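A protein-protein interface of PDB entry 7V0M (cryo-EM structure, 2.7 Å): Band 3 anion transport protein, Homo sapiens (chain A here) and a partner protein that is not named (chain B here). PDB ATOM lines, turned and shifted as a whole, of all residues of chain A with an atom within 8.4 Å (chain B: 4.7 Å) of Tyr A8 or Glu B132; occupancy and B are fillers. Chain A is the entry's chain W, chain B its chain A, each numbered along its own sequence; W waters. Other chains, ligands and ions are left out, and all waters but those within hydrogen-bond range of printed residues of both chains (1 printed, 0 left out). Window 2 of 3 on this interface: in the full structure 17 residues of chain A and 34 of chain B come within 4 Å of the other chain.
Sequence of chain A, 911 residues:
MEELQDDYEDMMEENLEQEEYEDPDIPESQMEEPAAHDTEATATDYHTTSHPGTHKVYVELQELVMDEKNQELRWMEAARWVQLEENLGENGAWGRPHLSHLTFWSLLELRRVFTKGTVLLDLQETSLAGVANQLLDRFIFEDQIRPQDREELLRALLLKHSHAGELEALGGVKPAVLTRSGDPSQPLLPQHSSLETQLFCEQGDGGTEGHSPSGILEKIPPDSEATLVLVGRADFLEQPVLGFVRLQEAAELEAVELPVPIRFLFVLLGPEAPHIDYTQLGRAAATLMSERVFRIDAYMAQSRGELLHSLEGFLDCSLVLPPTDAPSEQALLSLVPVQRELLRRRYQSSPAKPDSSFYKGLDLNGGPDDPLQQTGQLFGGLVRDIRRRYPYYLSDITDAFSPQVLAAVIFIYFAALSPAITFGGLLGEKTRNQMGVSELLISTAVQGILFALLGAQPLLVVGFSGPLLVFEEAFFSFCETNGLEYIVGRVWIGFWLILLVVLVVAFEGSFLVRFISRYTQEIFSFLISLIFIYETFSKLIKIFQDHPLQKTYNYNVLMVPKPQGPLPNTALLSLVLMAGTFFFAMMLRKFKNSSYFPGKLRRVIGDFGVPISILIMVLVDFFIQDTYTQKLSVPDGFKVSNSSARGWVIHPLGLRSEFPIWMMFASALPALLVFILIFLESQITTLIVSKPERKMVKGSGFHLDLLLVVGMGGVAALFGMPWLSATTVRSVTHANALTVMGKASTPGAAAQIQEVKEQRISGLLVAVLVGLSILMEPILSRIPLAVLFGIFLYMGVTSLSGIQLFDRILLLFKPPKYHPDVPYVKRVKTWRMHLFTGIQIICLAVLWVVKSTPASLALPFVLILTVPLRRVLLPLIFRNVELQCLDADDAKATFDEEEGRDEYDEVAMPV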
ATOM      1  N   GLU A   2      27.610   5.211 -13.108  1.00  0.00           N
ATOM      2  CA  GLU A   2      27.195   5.945 -11.918  1.00  0.00           C
ATOM      3  C   GLU A   2      25.674   6.016 -11.821  1.00  0.00           C
ATOM      4  O   GLU A   2      24.989   6.191 -12.830  1.00  0.00           O
ATOM      5  CB  GLU A   2      27.788   7.354 -11.922  1.00  0.00           C
ATOM      6  N   GLU A   3      25.161   5.854 -10.603  1.00  0.00           N
ATOM      7  CA  GLU A   3      23.749   5.918 -10.218  1.00  0.00           C
ATOM      8  C   GLU A   3      22.925   4.780 -10.813  1.00  0.00           C
ATOM      9  O   GLU A   3      21.712   4.730 -10.571  1.00  0.00           O
ATOM     10  CB  GLU A   3      23.086   7.254 -10.591  1.00  0.00           C
ATOM     11  N   LEU A   4      23.528   3.866 -11.578  1.00  0.00           N
ATOM     12  CA  LEU A   4      22.794   2.740 -12.140  1.00  0.00           C
ATOM     13  C   LEU A   4      23.540   1.422 -11.983  1.00  0.00           C
ATOM     14  O   LEU A   4      23.092   0.408 -12.534  1.00  0.00           O
ATOM     15  CB  LEU A   4      22.478   2.980 -13.621  1.00  0.00           C
ATOM     16  CG  LEU A   4      21.486   4.098 -13.943  1.00  0.00           C
ATOM     17  CD1 LEU A   4      21.433   4.351 -15.441  1.00  0.00           C
ATOM     18  CD2 LEU A   4      20.105   3.762 -13.400  1.00  0.00           C
ATOM     19  N   GLN A   5      24.659   1.401 -11.255  1.00  0.00           N
ATOM     20  CA  GLN A   5      25.410   0.164 -11.074  1.00  0.00           C
ATOM     21  C   GLN A   5      24.624  -0.859 -10.266  1.00  0.00           C
ATOM     22  O   GLN A   5      24.719  -2.061 -10.534  1.00  0.00           O
ATOM     23  CB  GLN A   5      26.750   0.455 -10.401  1.00  0.00           C
ATOM     24  N   ASP A   6      23.826  -0.403  -9.299  1.00  0.00           N
ATOM     25  CA  ASP A   6      23.068  -1.296  -8.431  1.00  0.00           C
ATOM     26  C   ASP A   6      21.967  -2.055  -9.163  1.00  0.00           C
ATOM     27  O   ASP A   6      21.385  -2.973  -8.578  1.00  0.00           O
ATOM     28  CB  ASP A   6      22.466  -0.504  -7.268  1.00  0.00           C
ATOM     29  N   ASP A   7      21.663  -1.692 -10.410  1.00  0.00           N
ATOM     30  CA  ASP A   7      20.694  -2.433 -11.209  1.00  0.00           C
ATOM     31  C   ASP A   7      21.190  -3.811 -11.626  1.00  0.00           C
ATOM     32  O   ASP A   7      20.390  -4.611 -12.121  1.00  0.00           O
ATOM     33  CB  ASP A   7      20.325  -1.640 -12.464  1.00  0.00           C
ATOM     34  CG  ASP A   7      19.377  -0.497 -12.178  1.00  0.00           C
ATOM     35  OD1 ASP A   7      19.162  -0.185 -10.991  1.00  0.00           O
ATOM     36  OD2 ASP A   7      18.847   0.093 -13.141  1.00  0.00           O
ATOM     37  N   TYR A   8      22.473  -4.108 -11.448  1.00  0.00           N
ATOM     38  CA  TYR A   8      23.071  -5.335 -11.949  1.00  0.00           C
ATOM     39  C   TYR A   8      23.210  -6.360 -10.832  1.00  0.00           C
ATOM     40  O   TYR A   8      23.318  -6.011  -9.653  1.00  0.00           O
ATOM     41  CB  TYR A   8      24.437  -5.065 -12.592  1.00  0.00           C
ATOM     42  CG  TYR A   8      24.385  -4.141 -13.790  1.00  0.00           C
ATOM     43  CD1 TYR A   8      24.152  -2.779 -13.641  1.00  0.00           C
ATOM     44  CD2 TYR A   8      24.552  -4.638 -15.075  1.00  0.00           C
ATOM     45  CE1 TYR A   8      24.097  -1.939 -14.733  1.00  0.00           C
ATOM     46  CE2 TYR A   8      24.499  -3.806 -16.173  1.00  0.00           C
ATOM     47  CZ  TYR A   8      24.272  -2.457 -15.996  1.00  0.00           C
ATOM     48  OH  TYR A   8      24.219  -1.620 -17.086  1.00  0.00           O
ATOM     49  N   GLU A   9      23.206  -7.636 -11.224  1.00  0.00           N
ATOM     50  CA  GLU A   9      23.178  -8.720 -10.250  1.00  0.00           C
ATOM     51  C   GLU A   9      24.469  -8.809  -9.448  1.00  0.00           C
ATOM     52  O   GLU A   9      24.429  -9.118  -8.253  1.00  0.00           O
ATOM     53  CB  GLU A   9      22.899 -10.048 -10.952  1.00  0.00           C
ATOM     54  CG  GLU A   9      21.628 -10.042 -11.776  1.00  0.00           C
ATOM     55  CD  GLU A   9      20.535 -10.884 -11.161  1.00  0.00           C
ATOM     56  OE1 GLU A   9      20.672 -11.260  -9.979  1.00  0.00           O
ATOM     57  OE2 GLU A   9      19.538 -11.170 -11.855  1.00  0.00           O
ATOM     58  N   ASP A  10      25.618  -8.562 -10.079  1.00  0.00           N
ATOM     59  CA  ASP A  10      26.880  -8.610  -9.347  1.00  0.00           C
ATOM     60  C   ASP A  10      26.954  -7.508  -8.296  1.00  0.00           C
ATOM     61  O   ASP A  10      27.383  -7.749  -7.159  1.00  0.00           O
ATOM     62  CB  ASP A  10      28.052  -8.504 -10.322  1.00  0.00           C
ATOM     63  CG  ASP A  10      28.074  -9.633 -11.330  1.00  0.00           C
ATOM     64  OD1 ASP A  10      27.494 -10.702 -11.041  1.00  0.00           O
ATOM     65  OD2 ASP A  10      28.672  -9.454 -12.411  1.00  0.00           O
ATOM     66  N   MET A  11      26.528  -6.295  -8.656  1.00  0.00           N
ATOM     67  CA  MET A  11      26.534  -5.193  -7.703  1.00  0.00           C
ATOM     68  C   MET A  11      25.572  -5.455  -6.552  1.00  0.00           C
ATOM     69  O   MET A  11      25.883  -5.154  -5.397  1.00  0.00           O
ATOM     70  CB  MET A  11      26.182  -3.886  -8.408  1.00  0.00           C
ATOM     71  CG  MET A  11      26.772  -2.583  -7.831  1.00  0.00           C
ATOM     72  SD  MET A  11      28.543  -2.477  -7.438  1.00  0.00           S
ATOM     73  CE  MET A  11      28.683  -3.242  -5.821  1.00  0.00           C
ATOM     74  N   MET A  12      24.396  -6.013  -6.850  1.00  0.00           N
ATOM     75  CA  MET A  12      23.445  -6.338  -5.793  1.00  0.00           C
ATOM     76  C   MET A  12      23.975  -7.442  -4.887  1.00  0.00           C
ATOM     77  O   MET A  12      23.772  -7.400  -3.669  1.00  0.00           O
ATOM     78  CB  MET A  12      22.100  -6.736  -6.395  1.00  0.00           C
ATOM     79  CG  MET A  12      20.923  -6.500  -5.463  1.00  0.00           C
ATOM     80  SD  MET A  12      21.133  -5.022  -4.456  1.00  0.00           S
ATOM     81  CE  MET A  12      20.241  -3.823  -5.434  1.00  0.00           C
ATOM     82  N   GLU A  13      24.647  -8.439  -5.463  1.00  0.00           N
ATOM     83  CA  GLU A  13      25.248  -9.496  -4.656  1.00  0.00           C
ATOM     84  C   GLU A  13      26.313  -8.932  -3.724  1.00  0.00           C
ATOM     85  O   GLU A  13      26.411  -9.334  -2.560  1.00  0.00           O
ATOM     86  CB  GLU A  13      25.840 -10.573  -5.562  1.00  0.00           C
ATOM     87  CG  GLU A  13      25.679 -11.984  -5.032  1.00  0.00           C
ATOM     88  CD  GLU A  13      26.824 -12.889  -5.435  1.00  0.00           C
ATOM     89  OE1 GLU A  13      27.210 -12.871  -6.622  1.00  0.00           O
ATOM     90  OE2 GLU A  13      27.343 -13.616  -4.562  1.00  0.00           O
ATOM     91  N   GLU A  14      27.126  -8.001  -4.225  1.00  0.00           N
ATOM     92  CA  GLU A  14      28.115  -7.357  -3.364  1.00  0.00           C
ATOM     93  C   GLU A  14      27.447  -6.502  -2.293  1.00  0.00           C
ATOM     94  O   GLU A  14      27.902  -6.469  -1.144  1.00  0.00           O
ATOM     95  CB  GLU A  14      29.076  -6.514  -4.201  1.00  0.00           C
ATOM     96  CG  GLU A  14      30.102  -7.325  -4.971  1.00  0.00           C
ATOM     97  CD  GLU A  14      31.406  -6.576  -5.176  1.00  0.00           C
ATOM     98  OE1 GLU A  14      31.358  -5.388  -5.560  1.00  0.00           O
ATOM     99  OE2 GLU A  14      32.478  -7.176  -4.953  1.00  0.00           O
ATOM    100  N   ASN A  15      26.366  -5.805  -2.650  1.00  0.00           N
ATOM    101  CA  ASN A  15      25.698  -4.915  -1.706  1.00  0.00           C
ATOM    102  C   ASN A  15      25.028  -5.692  -0.578  1.00  0.00           C
ATOM    103  O   ASN A  15      25.041  -5.251   0.577  1.00  0.00           O
ATOM    104  CB  ASN A  15      24.670  -4.051  -2.435  1.00  0.00           C
ATOM    105  CG  ASN A  15      25.307  -2.933  -3.236  1.00  0.00           C
ATOM    106  OD1 ASN A  15      26.296  -2.337  -2.813  1.00  0.00           O
ATOM    107  ND2 ASN A  15      24.732  -2.634  -4.392  1.00  0.00           N
ATOM    108  N   LYS B 128      23.363  -3.102 -26.280  1.00  0.00           N
ATOM    109  CA  LYS B 128      24.000  -3.467 -25.019  1.00  0.00           C
ATOM    110  C   LYS B 128      22.973  -3.611 -23.903  1.00  0.00           C
ATOM    111  O   LYS B 128      23.024  -4.565 -23.114  1.00  0.00           O
ATOM    112  CB  LYS B 128      25.058  -2.424 -24.656  1.00  0.00           C
ATOM    113  CG  LYS B 128      25.831  -2.725 -23.379  1.00  0.00           C
ATOM    114  CD  LYS B 128      26.589  -1.508 -22.860  1.00  0.00           C
ATOM    115  CE  LYS B 128      27.146  -0.646 -23.991  1.00  0.00           C
ATOM    116  NZ  LYS B 128      28.197  -1.345 -24.787  1.00  0.00           N
ATOM    117  N   PHE B 129      22.017  -2.680 -23.830  1.00  0.00           N
ATOM    118  CA  PHE B 129      20.994  -2.757 -22.792  1.00  0.00           C
ATOM    119  C   PHE B 129      20.089  -3.966 -22.989  1.00  0.00           C
ATOM    120  O   PHE B 129      19.701  -4.622 -22.015  1.00  0.00           O
ATOM    121  CB  PHE B 129      20.166  -1.474 -22.763  1.00  0.00           C
ATOM    122  CG  PHE B 129      19.138  -1.447 -21.669  1.00  0.00           C
ATOM    123  CD1 PHE B 129      19.509  -1.198 -20.361  1.00  0.00           C
ATOM    124  CD2 PHE B 129      17.804  -1.680 -21.949  1.00  0.00           C
ATOM    125  CE1 PHE B 129      18.568  -1.179 -19.352  1.00  0.00           C
ATOM    126  CE2 PHE B 129      16.860  -1.661 -20.946  1.00  0.00           C
ATOM    127  CZ  PHE B 129      17.241  -1.409 -19.646  1.00  0.00           C
ATOM    128  N   LEU B 130      19.727  -4.269 -24.236  1.00  0.00           N
ATOM    129  CA  LEU B 130      18.879  -5.425 -24.499  1.00  0.00           C
ATOM    130  C   LEU B 130      19.597  -6.724 -24.169  1.00  0.00           C
ATOM    131  O   LEU B 130      18.996  -7.638 -23.593  1.00  0.00           O
ATOM    132  CB  LEU B 130      18.419  -5.419 -25.955  1.00  0.00           C
ATOM    133  CG  LEU B 130      17.278  -4.460 -26.285  1.00  0.00           C
ATOM    134  CD1 LEU B 130      17.158  -4.282 -27.783  1.00  0.00           C
ATOM    135  CD2 LEU B 130      15.973  -4.958 -25.691  1.00  0.00           C
ATOM    136  N   LEU B 131      20.881  -6.824 -24.520  1.00  0.00           N
ATOM    137  CA  LEU B 131      21.651  -8.012 -24.168  1.00  0.00           C
ATOM    138  C   LEU B 131      21.763  -8.163 -22.658  1.00  0.00           C
ATOM    139  O   LEU B 131      21.647  -9.275 -22.130  1.00  0.00           O
ATOM    140  CB  LEU B 131      23.040  -7.953 -24.801  1.00  0.00           C
ATOM    141  CG  LEU B 131      23.114  -8.151 -26.314  1.00  0.00           C
ATOM    142  CD1 LEU B 131      24.503  -7.813 -26.815  1.00  0.00           C
ATOM    143  CD2 LEU B 131      22.722  -9.565 -26.700  1.00  0.00           C
ATOM    144  N   GLU B 132      21.972  -7.055 -21.943  1.00  0.00           N
ATOM    145  CA  GLU B 132      22.035  -7.115 -20.489  1.00  0.00           C
ATOM    146  C   GLU B 132      20.703  -7.484 -19.849  1.00  0.00           C
ATOM    147  O   GLU B 132      20.685  -7.838 -18.666  1.00  0.00           O
ATOM    148  CB  GLU B 132      22.520  -5.780 -19.926  1.00  0.00           C
ATOM    149  CG  GLU B 132      24.004  -5.526 -20.118  1.00  0.00           C
ATOM    150  CD  GLU B 132      24.398  -4.100 -19.790  1.00  0.00           C
ATOM    151  OE1 GLU B 132      25.527  -3.697 -20.141  1.00  0.00           O
ATOM    152  OE2 GLU B 132      23.577  -3.380 -19.185  1.00  0.00           O
ATOM    153  N   ASN B 133      19.596  -7.416 -20.588  1.00  0.00           N
ATOM    154  CA  ASN B 133      18.281  -7.748 -20.059  1.00  0.00           C
ATOM    155  C   ASN B 133      17.744  -9.060 -20.616  1.00  0.00           C
ATOM    156  O   ASN B 133      16.527  -9.269 -20.640  1.00  0.00           O
ATOM    157  CB  ASN B 133      17.296  -6.609 -20.322  1.00  0.00           C
ATOM    158  CG  ASN B 133      17.517  -5.430 -19.399  1.00  0.00           C
ATOM    159  OD1 ASN B 133      16.799  -5.253 -18.418  1.00  0.00           O
ATOM    160  ND2 ASN B 133      18.520  -4.620 -19.704  1.00  0.00           N
ATOM    161  N   GLY B 134      18.626  -9.951 -21.057  1.00  0.00           N
ATOM    162  CA  GLY B 134      18.207 -11.281 -21.448  1.00  0.00           C
ATOM    163  C   GLY B 134      17.629 -11.411 -22.836  1.00  0.00           C
ATOM    164  O   GLY B 134      16.851 -12.336 -23.087  1.00  0.00           O
ATOM    165  N   TYR B 166      29.594 -10.542 -26.104  1.00  0.00           N
ATOM    166  CA  TYR B 166      28.582 -10.923 -25.125  1.00  0.00           C
ATOM    167  C   TYR B 166      28.311 -12.422 -25.170  1.00  0.00           C
ATOM    168  O   TYR B 166      28.246 -13.080 -24.125  1.00  0.00           O
ATOM    169  CB  TYR B 166      27.295 -10.134 -25.367  1.00  0.00           C
ATOM    170  CG  TYR B 166      26.366 -10.098 -24.177  1.00  0.00           C
ATOM    171  CD1 TYR B 166      25.461 -11.125 -23.947  1.00  0.00           C
ATOM    172  CD2 TYR B 166      26.396  -9.038 -23.282  1.00  0.00           C
ATOM    173  CE1 TYR B 166      24.614 -11.097 -22.861  1.00  0.00           C
ATOM    174  CE2 TYR B 166      25.551  -9.001 -22.194  1.00  0.00           C
ATOM    175  CZ  TYR B 166      24.665 -10.034 -21.986  1.00  0.00           C
ATOM    176  OH  TYR B 166      23.821 -10.002 -20.904  1.00  0.00           O
ATOM    177  N   GLY B 170      23.757 -13.969 -20.937  1.00  0.00           N
ATOM    178  CA  GLY B 170      22.437 -13.968 -20.342  1.00  0.00           C
ATOM    179  C   GLY B 170      22.073 -12.673 -19.648  1.00  0.00           C
ATOM    180  O   GLY B 170      22.762 -11.661 -19.799  1.00  0.00           O
ATOM    181  N   LYS B 171      20.982 -12.694 -18.889  1.00  0.00           N
ATOM    182  CA  LYS B 171      20.547 -11.517 -18.150  1.00  0.00           C
ATOM    183  C   LYS B 171      21.480 -11.231 -16.984  1.00  0.00           C
ATOM    184  O   LYS B 171      21.538 -11.995 -16.017  1.00  0.00           O
ATOM    185  CB  LYS B 171      19.116 -11.722 -17.646  1.00  0.00           C
ATOM    186  CG  LYS B 171      18.323 -10.440 -17.507  1.00  0.00           C
ATOM    187  CD  LYS B 171      16.893 -10.717 -17.092  1.00  0.00           C
ATOM    188  CE  LYS B 171      16.273  -9.505 -16.424  1.00  0.00           C
ATOM    189  NZ  LYS B 171      15.070  -9.875 -15.633  1.00  0.00           N
ATOM    190  N   VAL B 172      22.213 -10.122 -17.078  1.00  0.00           N
ATOM    191  CA  VAL B 172      23.082  -9.660 -16.004  1.00  0.00           C
ATOM    192  C   VAL B 172      22.501  -8.468 -15.271  1.00  0.00           C
ATOM    193  O   VAL B 172      23.130  -7.965 -14.330  1.00  0.00           O
ATOM    194  CB  VAL B 172      24.492  -9.334 -16.524  1.00  0.00           C
ATOM    195  CG1 VAL B 172      25.173 -10.602 -17.002  1.00  0.00           C
ATOM    196  CG2 VAL B 172      24.424  -8.306 -17.638  1.00  0.00           C
ATOM    197  N   ARG B 173      21.327  -7.998 -15.670  1.00  0.00           N
ATOM    198  CA  ARG B 173      20.599  -6.976 -14.938  1.00  0.00           C
ATOM    199  C   ARG B 173      19.561  -7.636 -14.041  1.00  0.00           C
ATOM    200  O   ARG B 173      19.085  -8.740 -14.319  1.00  0.00           O
ATOM    201  CB  ARG B 173      19.916  -5.994 -15.890  1.00  0.00           C
ATOM    202  CG  ARG B 173      20.087  -4.541 -15.495  1.00  0.00           C
ATOM    203  CD  ARG B 173      19.450  -3.611 -16.502  1.00  0.00           C
ATOM    204  NE  ARG B 173      17.996  -3.628 -16.407  1.00  0.00           N
ATOM    205  CZ  ARG B 173      17.253  -2.567 -16.124  1.00  0.00           C
ATOM    206  NH1 ARG B 173      17.797  -1.385 -15.895  1.00  0.00           N
ATOM    207  NH2 ARG B 173      15.931  -2.699 -16.068  1.00  0.00           N
ATOM    208  N   LEU B 174      19.220  -6.948 -12.957  1.00  0.00           N
ATOM    209  CA  LEU B 174      18.235  -7.470 -12.029  1.00  0.00           C
ATOM    210  C   LEU B 174      16.860  -7.510 -12.693  1.00  0.00           C
ATOM    211  O   LEU B 174      16.612  -6.790 -13.665  1.00  0.00           O
ATOM    212  CB  LEU B 174      18.181  -6.605 -10.771  1.00  0.00           C
ATOM    213  CG  LEU B 174      19.256  -6.846  -9.712  1.00  0.00           C
ATOM    214  CD1 LEU B 174      19.290  -5.688  -8.732  1.00  0.00           C
ATOM    215  CD2 LEU B 174      19.025  -8.164  -8.991  1.00  0.00           C
HETATM  216  O   HOH W   1      26.265  -8.049 -13.467  1.00  0.00           O
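Water W1 lies within hydrogen-bond range of the side-chain carboxylate (OD2) of Asp A10 (3.0 Å) and the backbone carbonyl oxygen (O) of Val B172 (3.3 Å).
The side-chain amide oxygen (OD1) of Asn B133 sits at hydrogen-bond distance from the guanidinium group (NE) of Arg B173, at 2.8 Å.
O of Glu B132 is in hydrogen-bond range of N of Val B172 (3.2 Å).
The backbone carbonyl oxygen (O) of Glu B132 sits at hydrogen-bond distance from the backbone NH (N) of Arg B173 (3.1 Å).
Of the printed residues of chain B, Asp A6 touches Leu B174.
Tyr A8 touches two residues of chain B.
Printed residues of chain B within 4 Å of Glu A9: Val B172 (3.1 Å), Arg B173 (3.5 Å) and Leu B174 (3.6 Å).
Printed residues of chain B within 4 Å of Met A12: Leu B174 (3.7 Å).
Glu B132 touches just one residue of chain A: Tyr A8 (2.8 Å).
Asn B133 touches none of the printed residues of chain A.
Lys B171 touches none of the printed residues of chain A.
Of the printed residues of chain A, Val B172 touches Tyr A8 and Glu A9.
The nearest printed residue of chain A that does not touch Glu B132 is Glu A9 (7.3 Å).
Leu B174 touches Asp A6 (CD1 to O, 3.4 Å).
Tyr A8 touches Val B172.
Leu B174 touches Glu A9 (CD2 to OE1, 3.6 Å).
Leu B174 touches Met A12 (CD1 to CG, 3.7 Å).
Printed residues of chain B that touch a printed residue of chain A: Glu B132, Val B172, Arg B173 and Leu B174.
Hydrophobic or aromatic side chains of chain B within 4 Å of the printed part of chain A: Leu B174.
Along chain B the printed residues that touch a printed residue of chain A span positions 132 to 174.
Printed residues of chain A that touch a printed residue of chain B: Asp A6, Asp A7, Tyr A8, Glu A9 and Met A12.
Among the printed residues, 9 pairs touch across the chains.
Among the printed residues, Asp or Glu carboxylates within 4 Å of a Lys or Arg side-chain nitrogen of the other chain: Asp A7 with Arg B173.
OD2 of Asp A7 lies within salt-bridge range of NH1 of Arg B173 (3.3 Å).
OE2 of Glu A9 sits close to O of Arg B173 (3.5 Å).
The backbone NH (N) of Leu B174 lies within hydrogen-bond range of the backbone carbonyl oxygen (O) of Asp A7 (2.7 Å).
OE2 of Glu B132 lies within hydrogen-bond range of OH of Tyr A8 (2.8 Å).
The backbone NH of Glu A9 lies within hydrogen-bond range of the backbone carbonyl oxygen of Val B172, 3.1 Å away.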
